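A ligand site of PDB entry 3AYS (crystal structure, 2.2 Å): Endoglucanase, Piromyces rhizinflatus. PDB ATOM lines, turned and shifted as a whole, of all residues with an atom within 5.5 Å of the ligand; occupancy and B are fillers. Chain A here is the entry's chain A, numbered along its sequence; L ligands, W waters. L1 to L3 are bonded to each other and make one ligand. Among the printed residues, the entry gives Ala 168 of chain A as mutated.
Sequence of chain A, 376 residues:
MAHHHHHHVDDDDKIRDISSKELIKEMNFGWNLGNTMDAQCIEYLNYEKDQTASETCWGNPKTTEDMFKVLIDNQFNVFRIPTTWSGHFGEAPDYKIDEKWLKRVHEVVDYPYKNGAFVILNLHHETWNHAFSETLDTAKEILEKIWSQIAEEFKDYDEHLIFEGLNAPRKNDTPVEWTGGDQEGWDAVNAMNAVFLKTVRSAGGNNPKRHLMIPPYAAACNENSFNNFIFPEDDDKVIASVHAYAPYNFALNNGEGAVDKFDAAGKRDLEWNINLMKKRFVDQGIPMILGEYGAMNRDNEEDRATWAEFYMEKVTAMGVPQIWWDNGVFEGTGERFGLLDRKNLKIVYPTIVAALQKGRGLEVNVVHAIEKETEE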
ATOM      1  N   ASN A  35     -30.803  15.303  11.521  1.00  0.00           N
ATOM      2  CA  ASN A  35     -31.592  16.237  10.705  1.00  0.00           C
ATOM      3  C   ASN A  35     -32.893  15.599  10.135  1.00  0.00           C
ATOM      4  O   ASN A  35     -33.297  15.818   8.969  1.00  0.00           O
ATOM      5  CB  ASN A  35     -30.725  16.891   9.579  1.00  0.00           C
ATOM      6  CG  ASN A  35     -29.789  17.983  10.120  1.00  0.00           C
ATOM      7  OD1 ASN A  35     -29.533  18.076  11.336  1.00  0.00           O
ATOM      8  ND2 ASN A  35     -29.309  18.858   9.239  1.00  0.00           N
ATOM      9  N   ASP A  38     -35.314  14.925  14.519  1.00  0.00           N
ATOM     10  CA  ASP A  38     -34.830  16.088  15.276  1.00  0.00           C
ATOM     11  C   ASP A  38     -35.086  17.414  14.516  1.00  0.00           C
ATOM     12  O   ASP A  38     -35.011  18.492  15.118  1.00  0.00           O
ATOM     13  CB  ASP A  38     -33.340  15.932  15.558  1.00  0.00           C
ATOM     14  CG  ASP A  38     -32.559  15.487  14.343  1.00  0.00           C
ATOM     15  OD1 ASP A  38     -33.020  14.538  13.664  1.00  0.00           O
ATOM     16  OD2 ASP A  38     -31.489  16.049  14.030  1.00  0.00           O
ATOM     17  N   TRP A  58     -35.883  19.139   6.886  1.00  0.00           N
ATOM     18  CA  TRP A  58     -34.500  19.535   6.671  1.00  0.00           C
ATOM     19  C   TRP A  58     -33.900  18.806   5.509  1.00  0.00           C
ATOM     20  O   TRP A  58     -32.690  18.696   5.401  1.00  0.00           O
ATOM     21  CB  TRP A  58     -33.628  19.478   7.930  1.00  0.00           C
ATOM     22  CG  TRP A  58     -33.971  20.614   8.941  1.00  0.00           C
ATOM     23  CD1 TRP A  58     -34.772  21.709   8.704  1.00  0.00           C
ATOM     24  CD2 TRP A  58     -33.510  20.772  10.287  1.00  0.00           C
ATOM     25  NE1 TRP A  58     -34.845  22.507   9.808  1.00  0.00           N
ATOM     26  CE2 TRP A  58     -34.099  21.957  10.800  1.00  0.00           C
ATOM     27  CE3 TRP A  58     -32.649  20.027  11.115  1.00  0.00           C
ATOM     28  CZ2 TRP A  58     -33.857  22.421  12.096  1.00  0.00           C
ATOM     29  CZ3 TRP A  58     -32.402  20.482  12.401  1.00  0.00           C
ATOM     30  CH2 TRP A  58     -33.014  21.648  12.901  1.00  0.00           C
ATOM     31  N   ARG A  80     -28.861   5.821  16.661  1.00  0.00           N
ATOM     32  CA  ARG A  80     -29.495   6.878  17.473  1.00  0.00           C
ATOM     33  C   ARG A  80     -30.497   7.632  16.600  1.00  0.00           C
ATOM     34  O   ARG A  80     -30.225   7.947  15.413  1.00  0.00           O
ATOM     35  CB  ARG A  80     -28.423   7.852  17.993  1.00  0.00           C
ATOM     36  CG  ARG A  80     -28.911   8.995  18.918  1.00  0.00           C
ATOM     37  CD  ARG A  80     -27.706   9.460  19.755  1.00  0.00           C
ATOM     38  NE  ARG A  80     -27.884  10.658  20.595  1.00  0.00           N
ATOM     39  CZ  ARG A  80     -27.739  11.908  20.155  1.00  0.00           C
ATOM     40  NH1 ARG A  80     -27.513  12.169  18.872  1.00  0.00           N
ATOM     41  NH2 ARG A  80     -27.822  12.924  20.993  1.00  0.00           N
ATOM     42  N   HIS A 124     -34.311  16.064  21.741  1.00  0.00           N
ATOM     43  CA  HIS A 124     -33.183  16.646  20.999  1.00  0.00           C
ATOM     44  C   HIS A 124     -33.180  18.157  21.046  1.00  0.00           C
ATOM     45  O   HIS A 124     -32.838  18.737  22.069  1.00  0.00           O
ATOM     46  CB  HIS A 124     -33.111  16.117  19.566  1.00  0.00           C
ATOM     47  CG  HIS A 124     -31.735  16.166  18.994  1.00  0.00           C
ATOM     48  ND1 HIS A 124     -30.752  15.274  19.365  1.00  0.00           N
ATOM     49  CD2 HIS A 124     -31.152  17.033  18.139  1.00  0.00           C
ATOM     50  CE1 HIS A 124     -29.640  15.564  18.721  1.00  0.00           C
ATOM     51  NE2 HIS A 124     -29.848  16.624  17.954  1.00  0.00           N
ATOM     52  N   HIS A 125     -33.644  18.806  19.975  1.00  0.00           N
ATOM     53  CA  HIS A 125     -33.623  20.287  19.875  1.00  0.00           C
ATOM     54  C   HIS A 125     -34.861  20.892  20.573  1.00  0.00           C
ATOM     55  O   HIS A 125     -35.624  21.663  19.970  1.00  0.00           O
ATOM     56  CB  HIS A 125     -33.645  20.731  18.409  1.00  0.00           C
ATOM     57  CG  HIS A 125     -32.410  20.384  17.626  1.00  0.00           C
ATOM     58  ND1 HIS A 125     -31.132  20.588  18.106  1.00  0.00           N
ATOM     59  CD2 HIS A 125     -32.258  19.840  16.397  1.00  0.00           C
ATOM     60  CE1 HIS A 125     -30.256  20.202  17.198  1.00  0.00           C
ATOM     61  NE2 HIS A 125     -30.914  19.745  16.145  1.00  0.00           N
ATOM     62  N   ASN A 167     -30.326  15.923  25.217  1.00  0.00           N
ATOM     63  CA  ASN A 167     -29.288  15.836  24.193  1.00  0.00           C
ATOM     64  C   ASN A 167     -28.062  16.605  24.658  1.00  0.00           C
ATOM     65  O   ASN A 167     -27.101  16.029  25.156  1.00  0.00           O
ATOM     66  CB  ASN A 167     -29.827  16.377  22.850  1.00  0.00           C
ATOM     67  CG  ASN A 167     -28.745  16.468  21.764  1.00  0.00           C
ATOM     68  OD1 ASN A 167     -27.986  15.514  21.557  1.00  0.00           O
ATOM     69  ND2 ASN A 167     -28.680  17.605  21.065  1.00  0.00           N
ATOM     70  N   ALA A 168     -28.125  17.925  24.544  1.00  0.00           N
ATOM     71  CA  ALA A 168     -27.000  18.827  24.850  1.00  0.00           C
ATOM     72  C   ALA A 168     -27.536  20.051  25.627  1.00  0.00           C
ATOM     73  O   ALA A 168     -27.450  21.202  25.150  1.00  0.00           O
ATOM     74  CB  ALA A 168     -26.328  19.261  23.539  1.00  0.00           C
ATOM     75  N   TRP A 178     -21.282  27.058  25.097  1.00  0.00           N
ATOM     76  CA  TRP A 178     -20.448  26.029  24.516  1.00  0.00           C
ATOM     77  C   TRP A 178     -19.112  25.791  25.216  1.00  0.00           C
ATOM     78  O   TRP A 178     -18.442  24.798  24.922  1.00  0.00           O
ATOM     79  CB  TRP A 178     -20.226  26.319  23.032  1.00  0.00           C
ATOM     80  CG  TRP A 178     -21.482  26.120  22.161  1.00  0.00           C
ATOM     81  CD1 TRP A 178     -22.099  27.059  21.381  1.00  0.00           C
ATOM     82  CD2 TRP A 178     -22.215  24.896  21.982  1.00  0.00           C
ATOM     83  NE1 TRP A 178     -23.193  26.491  20.733  1.00  0.00           N
ATOM     84  CE2 TRP A 178     -23.268  25.170  21.087  1.00  0.00           C
ATOM     85  CE3 TRP A 178     -22.061  23.591  22.471  1.00  0.00           C
ATOM     86  CZ2 TRP A 178     -24.187  24.178  20.667  1.00  0.00           C
ATOM     87  CZ3 TRP A 178     -22.982  22.638  22.095  1.00  0.00           C
ATOM     88  CH2 TRP A 178     -24.041  22.935  21.208  1.00  0.00           C
ATOM     89  N   HIS A 243     -20.707  14.065  23.404  1.00  0.00           N
ATOM     90  CA  HIS A 243     -20.527  14.333  22.001  1.00  0.00           C
ATOM     91  C   HIS A 243     -19.127  14.934  21.789  1.00  0.00           C
ATOM     92  O   HIS A 243     -18.719  15.836  22.537  1.00  0.00           O
ATOM     93  CB  HIS A 243     -21.571  15.377  21.544  1.00  0.00           C
ATOM     94  CG  HIS A 243     -22.985  14.903  21.705  1.00  0.00           C
ATOM     95  ND1 HIS A 243     -24.064  15.734  21.588  1.00  0.00           N
ATOM     96  CD2 HIS A 243     -23.471  13.655  21.970  1.00  0.00           C
ATOM     97  CE1 HIS A 243     -25.175  15.029  21.790  1.00  0.00           C
ATOM     98  NE2 HIS A 243     -24.841  13.763  22.024  1.00  0.00           N
ATOM     99  N   TYR A 245     -16.869  16.180  18.633  1.00  0.00           N
ATOM    100  CA  TYR A 245     -16.402  16.386  17.282  1.00  0.00           C
ATOM    101  C   TYR A 245     -14.978  16.908  17.305  1.00  0.00           C
ATOM    102  O   TYR A 245     -14.708  18.013  16.886  1.00  0.00           O
ATOM    103  CB  TYR A 245     -17.287  17.411  16.581  1.00  0.00           C
ATOM    104  CG  TYR A 245     -18.737  16.949  16.409  1.00  0.00           C
ATOM    105  CD1 TYR A 245     -19.168  16.329  15.228  1.00  0.00           C
ATOM    106  CD2 TYR A 245     -19.656  17.093  17.457  1.00  0.00           C
ATOM    107  CE1 TYR A 245     -20.529  15.938  15.053  1.00  0.00           C
ATOM    108  CE2 TYR A 245     -20.996  16.689  17.315  1.00  0.00           C
ATOM    109  CZ  TYR A 245     -21.421  16.156  16.097  1.00  0.00           C
ATOM    110  OH  TYR A 245     -22.722  15.801  15.968  1.00  0.00           O
ATOM    111  N   LEU A 252     -15.338  20.102  12.734  1.00  0.00           N
ATOM    112  CA  LEU A 252     -16.585  20.850  12.858  1.00  0.00           C
ATOM    113  C   LEU A 252     -16.437  22.343  12.503  1.00  0.00           C
ATOM    114  O   LEU A 252     -17.388  22.945  12.017  1.00  0.00           O
ATOM    115  CB  LEU A 252     -17.140  20.676  14.291  1.00  0.00           C
ATOM    116  CG  LEU A 252     -18.456  21.380  14.637  1.00  0.00           C
ATOM    117  CD1 LEU A 252     -19.556  21.197  13.622  1.00  0.00           C
ATOM    118  CD2 LEU A 252     -18.945  20.911  15.986  1.00  0.00           C
ATOM    119  N   GLU A 292     -22.349  11.218  19.574  1.00  0.00           N
ATOM    120  CA  GLU A 292     -22.195  11.982  18.324  1.00  0.00           C
ATOM    121  C   GLU A 292     -20.722  12.315  18.158  1.00  0.00           C
ATOM    122  O   GLU A 292     -20.023  12.662  19.158  1.00  0.00           O
ATOM    123  CB  GLU A 292     -22.943  13.342  18.326  1.00  0.00           C
ATOM    124  CG  GLU A 292     -24.448  13.335  18.464  1.00  0.00           C
ATOM    125  CD  GLU A 292     -25.083  14.705  18.276  1.00  0.00           C
ATOM    126  OE1 GLU A 292     -24.383  15.689  17.857  1.00  0.00           O
ATOM    127  OE2 GLU A 292     -26.290  14.839  18.597  1.00  0.00           O
ATOM    128  N   TRP A 325     -22.388  11.082  13.414  1.00  0.00           N
ATOM    129  CA  TRP A 325     -23.450  12.071  13.180  1.00  0.00           C
ATOM    130  C   TRP A 325     -23.688  12.270  11.694  1.00  0.00           C
ATOM    131  O   TRP A 325     -22.790  12.741  10.986  1.00  0.00           O
ATOM    132  CB  TRP A 325     -23.141  13.422  13.825  1.00  0.00           C
ATOM    133  CG  TRP A 325     -24.198  14.441  13.526  1.00  0.00           C
ATOM    134  CD1 TRP A 325     -24.114  15.528  12.720  1.00  0.00           C
ATOM    135  CD2 TRP A 325     -25.525  14.441  14.077  1.00  0.00           C
ATOM    136  NE1 TRP A 325     -25.329  16.216  12.722  1.00  0.00           N
ATOM    137  CE2 TRP A 325     -26.205  15.552  13.537  1.00  0.00           C
ATOM    138  CE3 TRP A 325     -26.195  13.604  14.995  1.00  0.00           C
ATOM    139  CZ2 TRP A 325     -27.563  15.854  13.886  1.00  0.00           C
ATOM    140  CZ3 TRP A 325     -27.524  13.917  15.348  1.00  0.00           C
ATOM    141  CH2 TRP A 325     -28.192  15.018  14.793  1.00  0.00           C
ATOM    142  N   ASN A 327     -26.035  13.971   8.976  1.00  0.00           N
ATOM    143  CA  ASN A 327     -27.142  14.899   8.880  1.00  0.00           C
ATOM    144  C   ASN A 327     -27.733  14.889   7.489  1.00  0.00           C
ATOM    145  O   ASN A 327     -28.603  15.702   7.183  1.00  0.00           O
ATOM    146  CB  ASN A 327     -26.759  16.335   9.289  1.00  0.00           C
ATOM    147  CG  ASN A 327     -25.677  16.928   8.443  1.00  0.00           C
ATOM    148  OD1 ASN A 327     -25.016  16.245   7.645  1.00  0.00           O
ATOM    149  ND2 ASN A 327     -25.434  18.187   8.653  1.00  0.00           N
ATOM    150  N   VAL A 329     -26.075  15.766   4.775  1.00  0.00           N
ATOM    151  CA  VAL A 329     -25.628  16.924   3.974  1.00  0.00           C
ATOM    152  C   VAL A 329     -24.220  16.644   3.413  1.00  0.00           C
ATOM    153  O   VAL A 329     -23.320  16.211   4.158  1.00  0.00           O
ATOM    154  CB  VAL A 329     -25.568  18.239   4.807  1.00  0.00           C
ATOM    155  CG1 VAL A 329     -24.941  19.398   3.949  1.00  0.00           C
ATOM    156  CG2 VAL A 329     -26.953  18.707   5.327  1.00  0.00           C
ATOM    157  N   GLU A 335     -22.869  22.384   7.540  1.00  0.00           N
ATOM    158  CA  GLU A 335     -22.155  21.208   8.064  1.00  0.00           C
ATOM    159  C   GLU A 335     -22.351  19.977   7.200  1.00  0.00           C
ATOM    160  O   GLU A 335     -23.483  19.576   6.970  1.00  0.00           O
ATOM    161  CB  GLU A 335     -22.567  20.940   9.518  1.00  0.00           C
ATOM    162  CG  GLU A 335     -22.446  22.203  10.358  1.00  0.00           C
ATOM    163  CD  GLU A 335     -22.960  22.027  11.762  1.00  0.00           C
ATOM    164  OE1 GLU A 335     -23.428  20.946  12.156  1.00  0.00           O
ATOM    165  OE2 GLU A 335     -22.831  22.987  12.507  1.00  0.00           O
ATOM    166  N   PHE A 337     -22.000  16.473   7.077  1.00  0.00           N
ATOM    167  CA  PHE A 337     -21.714  15.232   7.783  1.00  0.00           C
ATOM    168  C   PHE A 337     -22.303  13.957   7.149  1.00  0.00           C
ATOM    169  O   PHE A 337     -22.240  12.911   7.724  1.00  0.00           O
ATOM    170  CB  PHE A 337     -22.146  15.308   9.258  1.00  0.00           C
ATOM    171  CG  PHE A 337     -21.255  16.205  10.088  1.00  0.00           C
ATOM    172  CD1 PHE A 337     -19.975  15.806  10.461  1.00  0.00           C
ATOM    173  CD2 PHE A 337     -21.728  17.435  10.534  1.00  0.00           C
ATOM    174  CE1 PHE A 337     -19.156  16.624  11.249  1.00  0.00           C
ATOM    175  CE2 PHE A 337     -20.932  18.290  11.337  1.00  0.00           C
ATOM    176  CZ  PHE A 337     -19.630  17.863  11.675  1.00  0.00           C
HETATM  177  C1  LIG L   1     -26.419  18.484  18.024  1.00  0.00           C
HETATM  178  C2  LIG L   1     -26.658  18.183  16.540  1.00  0.00           C
HETATM  179  C3  LIG L   1     -25.879  19.159  15.657  1.00  0.00           C
HETATM  180  C4  LIG L   1     -24.412  18.891  16.039  1.00  0.00           C
HETATM  181  C5  LIG L   1     -23.417  19.480  15.035  1.00  0.00           C
HETATM  182  C6  LIG L   1     -24.932  18.788  18.390  1.00  0.00           C
HETATM  183  O1  LIG L   1     -24.861  19.583  19.596  1.00  0.00           O
HETATM  184  O2  LIG L   1     -26.924  17.391  18.840  1.00  0.00           O
HETATM  185  O3  LIG L   1     -28.055  18.353  16.321  1.00  0.00           O
HETATM  186  O4  LIG L   1     -26.035  18.920  14.266  1.00  0.00           O
HETATM  187  O5  LIG L   1     -24.299  19.511  17.324  1.00  0.00           O
HETATM  188  O6  LIG L   1     -23.646  20.907  15.039  1.00  0.00           O
HETATM  189  C1  LG2 L   2     -26.534  19.664  12.135  1.00  0.00           C
HETATM  190  C2  LG2 L   2     -26.922  20.895  11.318  1.00  0.00           C
HETATM  191  C3  LG2 L   2     -28.236  21.456  11.806  1.00  0.00           C
HETATM  192  C4  LG2 L   2     -28.055  21.718  13.299  1.00  0.00           C
HETATM  193  C5  LG2 L   2     -29.225  22.463  13.920  1.00  0.00           C
HETATM  194  C6  LG2 L   2     -26.427  20.094  13.591  1.00  0.00           C
HETATM  195  O1  LG2 L   2     -25.311  19.112  11.585  1.00  0.00           O
HETATM  196  O2  LG2 L   2     -27.023  20.513   9.952  1.00  0.00           O
HETATM  197  O3  LG2 L   2     -28.414  22.675  11.100  1.00  0.00           O
HETATM  198  O4  LG2 L   2     -27.743  20.519  14.020  1.00  0.00           O
HETATM  199  O5  LG2 L   2     -28.769  22.679  15.271  1.00  0.00           O
HETATM  200  C1  LG3 L   3     -29.738  24.413  10.390  1.00  0.00           C
HETATM  201  C2  LG3 L   3     -31.033  24.700   9.674  1.00  0.00           C
HETATM  202  C3  LG3 L   3     -30.947  24.053   8.326  1.00  0.00           C
HETATM  203  C4  LG3 L   3     -30.839  22.559   8.559  1.00  0.00           C
HETATM  204  C5  LG3 L   3     -30.909  21.750   7.286  1.00  0.00           C
HETATM  205  C6  LG3 L   3     -29.667  22.915  10.518  1.00  0.00           C
HETATM  206  O1  LG3 L   3     -29.816  24.952  11.708  1.00  0.00           O
HETATM  207  O2  LG3 L   3     -31.240  26.105   9.535  1.00  0.00           O
HETATM  208  O3  LG3 L   3     -32.314  24.197   8.012  1.00  0.00           O
HETATM  209  O4  LG3 L   3     -29.615  22.341   9.219  1.00  0.00           O
HETATM  210  O5  LG3 L   3     -29.902  22.234   6.434  1.00  0.00           O
HETATM  211  O   HOH W   1     -27.404  22.480  17.516  1.00  0.00           O
HETATM  212  O   HOH W   2     -26.524  25.290  11.893  1.00  0.00           O
HETATM  213  O   HOH W   3     -23.567  18.225  21.570  1.00  0.00           O
HETATM  214  O   HOH W   4     -27.154  21.061  19.997  1.00  0.00           O
HETATM  215  O   HOH W   5     -26.203  22.428   8.165  1.00  0.00           O
HETATM  216  O   HOH W   6     -31.557  23.812  16.121  1.00  0.00           O
HETATM  217  O   HOH W   7     -29.891  18.267  13.991  1.00  0.00           O
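NE1 of Trp 58 touches O3 of LG3 L3, at 3.5 Å. CH2 of Trp 178 touches O1 of LIG L1 (3.8 Å). Tyr 245 touches the ligand. Hydrophobic or aromatic side chains that line the ligand: Trp 58, His 124, His 125, Trp 178 and Trp 325. Within 4 Å of the ligand: Asn 35, Trp 58, His 124, His 125, Asn 167, Trp 178, Tyr 245, Glu 292, Trp 325, Asn 327 and Glu 335.
O2 of LIG L1 lies within hydrogen-bond range of OE2 of Glu 292 (2.6 Å). The side-chain carboxylate (OE1) of Glu 335 sits at hydrogen-bond distance from an oxygen (O1) of LG2 L2 (2.7 Å). The side-chain amide nitrogen of Asn 167 lies within hydrogen-bond range of an oxygen (O2) of LIG L1, 2.8 Å away. An oxygen (O2) of LG2 L2 sits at hydrogen-bond distance from the side-chain amide nitrogen (ND2) of Asn 35 (2.9 Å). A ring nitrogen (NE2) of His 124 sits at hydrogen-bond distance from an oxygen (O3) of LIG L1 (3.0 Å). A ring nitrogen (NE2) of His 125 sits close to an oxygen (O3) of LIG L1 (3.2 Å). ND2 of Asn 327 lies within hydrogen-bond range of O1 of LG2 L2 (3.1 Å). An oxygen (O1) of LG2 L2 sits at hydrogen-bond distance from the indole nitrogen (NE1) of Trp 325.
Water W3 bridges a ring nitrogen (ND1) of His 243 (2.5 Å) and an oxygen (O1) of LIG L1 (2.7 Å). Water W5 bridges an oxygen (O2) of LG2 L2 (2.7 Å) and the backbone NH of Glu 335 (3.4 Å). Water W7 lies within hydrogen-bond range of the side-chain amide oxygen of Asn 35, the side-chain carboxylate of Asp 38, a ring nitrogen (NE2) of His 125 and an oxygen (O3) of LIG L1.
OD1 of Asn 167 sits close to OE2 of Glu 292, at 3.5 Å. The side-chain carboxylate of Glu 292 lies within hydrogen-bond range of the side-chain hydroxyl of Tyr 245. The side-chain carboxylate (OE2) of Glu 292 is in salt-bridge range of the guanidinium group (NH1) of Arg 80. The backbone carbonyl oxygen of Glu 335 lies within hydrogen-bond range of the side-chain amide nitrogen of Asn 327, at 2.9 Å. NH2 of Arg 80 lies within hydrogen-bond range of OD1 of Asn 167 (2.7 Å). N of Asn 35 lies within hydrogen-bond range of OD2 of Asp 38 (2.7 Å). The side-chain amide oxygen (OD1) of Asn 327 sits at hydrogen-bond distance from the backbone NH (N) of Phe 337 (3.1 Å). The backbone NH (N) of Val 329 sits at hydrogen-bond distance from the side-chain amide oxygen (OD1) of Asn 327, at 3.1 Å.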
